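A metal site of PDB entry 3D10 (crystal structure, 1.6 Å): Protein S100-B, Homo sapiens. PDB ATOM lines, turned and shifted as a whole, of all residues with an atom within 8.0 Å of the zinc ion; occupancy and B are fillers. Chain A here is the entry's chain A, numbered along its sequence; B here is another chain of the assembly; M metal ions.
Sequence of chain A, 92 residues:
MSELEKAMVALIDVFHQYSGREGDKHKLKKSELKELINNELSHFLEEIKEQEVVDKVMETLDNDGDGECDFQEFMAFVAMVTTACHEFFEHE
Of the 11 residues printed, 4 come within 4 Å of the zinc ion.
The side-chain carboxylate of Glu 90 of chain B lies close to a ring nitrogen (NE2) of His 86 of chain B, at 2.9 Å. A ring nitrogen (ND1) of His 16 is in hydrogen-bond range of the backbone carbonyl oxygen (O) of Ile 12 (3.4 Å). A ring nitrogen (NE2) of His 26 lies close to the side-chain carboxylate (OE2) of Glu 90 of chain B, at 3.2 Å.
The zinc ion is bound by NE2 of His 26, NE2 of His 16 and NE2 of His 86 of chain B. Slightly farther from the zinc ion lies OE1 of Glu 90 of chain B (2.6 Å). Slightly farther from the zinc ion lies the side-chain carboxylate (OE2) of Glu 90 of chain B (2.7 Å).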
ATOM      1  N   ILE A  12       6.807  -3.279 -13.551  1.00  0.00           N
ATOM      2  CA  ILE A  12       5.823  -3.560 -14.563  1.00  0.00           C
ATOM      3  C   ILE A  12       6.508  -4.038 -15.823  1.00  0.00           C
ATOM      4  O   ILE A  12       6.077  -5.000 -16.440  1.00  0.00           O
ATOM      5  CB  ILE A  12       5.047  -2.321 -14.929  1.00  0.00           C
ATOM      6  CG1 ILE A  12       4.118  -1.853 -13.771  1.00  0.00           C
ATOM      7  CG2 ILE A  12       4.263  -2.563 -16.273  1.00  0.00           C
ATOM      8  CD1 ILE A  12       3.453  -0.534 -14.142  1.00  0.00           C
ATOM      9  N   PHE A  15       7.939  -7.760 -15.386  1.00  0.00           N
ATOM     10  CA  PHE A  15       6.801  -8.690 -15.497  1.00  0.00           C
ATOM     11  C   PHE A  15       6.441  -8.972 -16.985  1.00  0.00           C
ATOM     12  O   PHE A  15       6.138 -10.106 -17.399  1.00  0.00           O
ATOM     13  CB  PHE A  15       5.524  -8.147 -14.791  1.00  0.00           C
ATOM     14  CG  PHE A  15       4.334  -9.088 -14.886  1.00  0.00           C
ATOM     15  CD1 PHE A  15       4.282 -10.259 -14.075  1.00  0.00           C
ATOM     16  CD2 PHE A  15       3.280  -8.865 -15.761  1.00  0.00           C
ATOM     17  CE1 PHE A  15       3.185 -11.120 -14.161  1.00  0.00           C
ATOM     18  CE2 PHE A  15       2.237  -9.731 -15.855  1.00  0.00           C
ATOM     19  CZ  PHE A  15       2.159 -10.863 -15.063  1.00  0.00           C
ATOM     20  N   HIS A  16       6.375  -7.916 -17.796  1.00  0.00           N
ATOM     21  CA  HIS A  16       5.852  -8.051 -19.121  1.00  0.00           C
ATOM     22  C   HIS A  16       6.892  -8.713 -20.024  1.00  0.00           C
ATOM     23  O   HIS A  16       6.555  -9.423 -20.964  1.00  0.00           O
ATOM     24  CB  HIS A  16       5.581  -6.657 -19.710  1.00  0.00           C
ATOM     25  CG  HIS A  16       4.300  -6.020 -19.260  1.00  0.00           C
ATOM     26  ND1 HIS A  16       4.141  -4.648 -19.227  1.00  0.00           N
ATOM     27  CD2 HIS A  16       3.101  -6.555 -18.904  1.00  0.00           C
ATOM     28  CE1 HIS A  16       2.911  -4.370 -18.824  1.00  0.00           C
ATOM     29  NE2 HIS A  16       2.257  -5.511 -18.636  1.00  0.00           N
ATOM     30  N   SER A  19       6.350 -12.412 -18.901  1.00  0.00           N
ATOM     31  CA  SER A  19       4.984 -12.958 -19.158  1.00  0.00           C
ATOM     32  C   SER A  19       4.559 -13.080 -20.648  1.00  0.00           C
ATOM     33  O   SER A  19       3.789 -13.971 -21.008  1.00  0.00           O
ATOM     34  CB  SER A  19       3.956 -12.166 -18.334  1.00  0.00           C
ATOM     35  OG  SER A  19       3.722 -10.876 -18.908  1.00  0.00           O
ATOM     36  N   LYS A  25      -0.096 -13.850 -22.577  1.00  0.00           N
ATOM     37  CA  LYS A  25       0.969 -12.856 -22.532  1.00  0.00           C
ATOM     38  C   LYS A  25       1.037 -12.025 -21.244  1.00  0.00           C
ATOM     39  O   LYS A  25       1.950 -11.221 -21.080  1.00  0.00           O
ATOM     40  CB  LYS A  25       0.944 -11.944 -23.741  1.00  0.00           C
ATOM     41  CG  LYS A  25       1.394 -12.659 -24.987  1.00  0.00           C
ATOM     42  CD  LYS A  25       1.695 -11.692 -26.113  1.00  0.00           C
ATOM     43  CE  LYS A  25       2.358 -12.424 -27.266  1.00  0.00           C
ATOM     44  NZ  LYS A  25       1.514 -13.437 -27.970  1.00  0.00           N
ATOM     45  N   HIS A  26       0.049 -12.182 -20.366  1.00  0.00           N
ATOM     46  CA  HIS A  26      -0.085 -11.375 -19.154  1.00  0.00           C
ATOM     47  C   HIS A  26       0.039 -12.247 -17.883  1.00  0.00           C
ATOM     48  O   HIS A  26      -0.360 -11.834 -16.790  1.00  0.00           O
ATOM     49  CB  HIS A  26      -1.452 -10.678 -19.172  1.00  0.00           C
ATOM     50  CG  HIS A  26      -1.414  -9.214 -18.846  1.00  0.00           C
ATOM     51  ND1 HIS A  26      -2.537  -8.523 -18.438  1.00  0.00           N
ATOM     52  CD2 HIS A  26      -0.407  -8.307 -18.886  1.00  0.00           C
ATOM     53  CE1 HIS A  26      -2.210  -7.252 -18.237  1.00  0.00           C
ATOM     54  NE2 HIS A  26      -0.923  -7.110 -18.478  1.00  0.00           N
ATOM     55  N   PHE A  71      -0.213 -10.573 -12.723  1.00  0.00           N
ATOM     56  CA  PHE A  71       0.409  -9.381 -12.151  1.00  0.00           C
ATOM     57  C   PHE A  71       0.248  -9.198 -10.612  1.00  0.00           C
ATOM     58  O   PHE A  71       1.184  -8.905  -9.899  1.00  0.00           O
ATOM     59  CB  PHE A  71      -0.086  -8.104 -12.894  1.00  0.00           C
ATOM     60  CG  PHE A  71       0.553  -6.882 -12.409  1.00  0.00           C
ATOM     61  CD1 PHE A  71       1.841  -6.556 -12.854  1.00  0.00           C
ATOM     62  CD2 PHE A  71      -0.061  -6.061 -11.479  1.00  0.00           C
ATOM     63  CE1 PHE A  71       2.498  -5.409 -12.354  1.00  0.00           C
ATOM     64  CE2 PHE A  71       0.585  -4.925 -10.986  1.00  0.00           C
ATOM     65  CZ  PHE A  71       1.859  -4.601 -11.433  1.00  0.00           C
ATOM     66  N   HIS B  86       0.017   0.489 -14.025  1.00  0.00           N
ATOM     67  CA  HIS B  86      -0.133  -0.570 -15.007  1.00  0.00           C
ATOM     68  C   HIS B  86      -1.429  -0.520 -15.815  1.00  0.00           C
ATOM     69  O   HIS B  86      -1.445  -0.547 -17.064  1.00  0.00           O
ATOM     70  CB  HIS B  86       0.045  -1.888 -14.282  1.00  0.00           C
ATOM     71  CG  HIS B  86      -0.300  -3.068 -15.100  1.00  0.00           C
ATOM     72  ND1 HIS B  86      -1.152  -4.055 -14.672  1.00  0.00           N
ATOM     73  CD2 HIS B  86       0.158  -3.460 -16.308  1.00  0.00           C
ATOM     74  CE1 HIS B  86      -1.224  -4.998 -15.591  1.00  0.00           C
ATOM     75  NE2 HIS B  86      -0.465  -4.645 -16.616  1.00  0.00           N
ATOM     76  N   GLU B  87      -2.537  -0.365 -15.133  1.00  0.00           N
ATOM     77  CA  GLU B  87      -3.796  -0.212 -15.791  1.00  0.00           C
ATOM     78  C   GLU B  87      -3.932   1.097 -16.584  1.00  0.00           C
ATOM     79  O   GLU B  87      -4.605   1.144 -17.633  1.00  0.00           O
ATOM     80  CB  GLU B  87      -4.893  -0.243 -14.749  1.00  0.00           C
ATOM     81  CG  GLU B  87      -5.157  -1.627 -14.186  1.00  0.00           C
ATOM     82  CD  GLU B  87      -5.946  -1.570 -12.896  1.00  0.00           C
ATOM     83  OE1 GLU B  87      -6.545  -0.497 -12.644  1.00  0.00           O
ATOM     84  OE2 GLU B  87      -5.931  -2.563 -12.117  1.00  0.00           O
ATOM     85  N   PHE B  89      -1.905   2.584 -18.376  1.00  0.00           N
ATOM     86  CA  PHE B  89      -1.267   2.560 -19.713  1.00  0.00           C
ATOM     87  C   PHE B  89      -1.687   1.423 -20.601  1.00  0.00           C
ATOM     88  O   PHE B  89      -1.142   1.226 -21.717  1.00  0.00           O
ATOM     89  CB  PHE B  89       0.254   2.668 -19.608  1.00  0.00           C
ATOM     90  CG  PHE B  89       0.703   4.020 -19.175  1.00  0.00           C
ATOM     91  CD1 PHE B  89       0.957   5.007 -20.129  1.00  0.00           C
ATOM     92  CD2 PHE B  89       0.858   4.307 -17.818  1.00  0.00           C
ATOM     93  CE1 PHE B  89       1.364   6.260 -19.730  1.00  0.00           C
ATOM     94  CE2 PHE B  89       1.261   5.577 -17.410  1.00  0.00           C
ATOM     95  CZ  PHE B  89       1.513   6.550 -18.381  1.00  0.00           C
ATOM     96  N   GLU B  90      -2.758   0.774 -20.148  1.00  0.00           N
ATOM     97  CA  GLU B  90      -3.401  -0.359 -20.835  1.00  0.00           C
ATOM     98  C   GLU B  90      -4.852  -0.060 -21.152  1.00  0.00           C
ATOM     99  O   GLU B  90      -5.517   0.737 -20.458  1.00  0.00           O
ATOM    100  CB  GLU B  90      -3.374  -1.573 -19.929  1.00  0.00           C
ATOM    101  CG  GLU B  90      -2.933  -2.822 -20.576  1.00  0.00           C
ATOM    102  CD  GLU B  90      -1.953  -3.523 -19.702  1.00  0.00           C
ATOM    103  OE1 GLU B  90      -0.744  -3.336 -19.914  1.00  0.00           O
ATOM    104  OE2 GLU B  90      -2.380  -4.243 -18.786  1.00  0.00           O
HETATM  105 ZN    ZN M   1       0.083  -5.449 -18.584  1.00  0.00          ZN
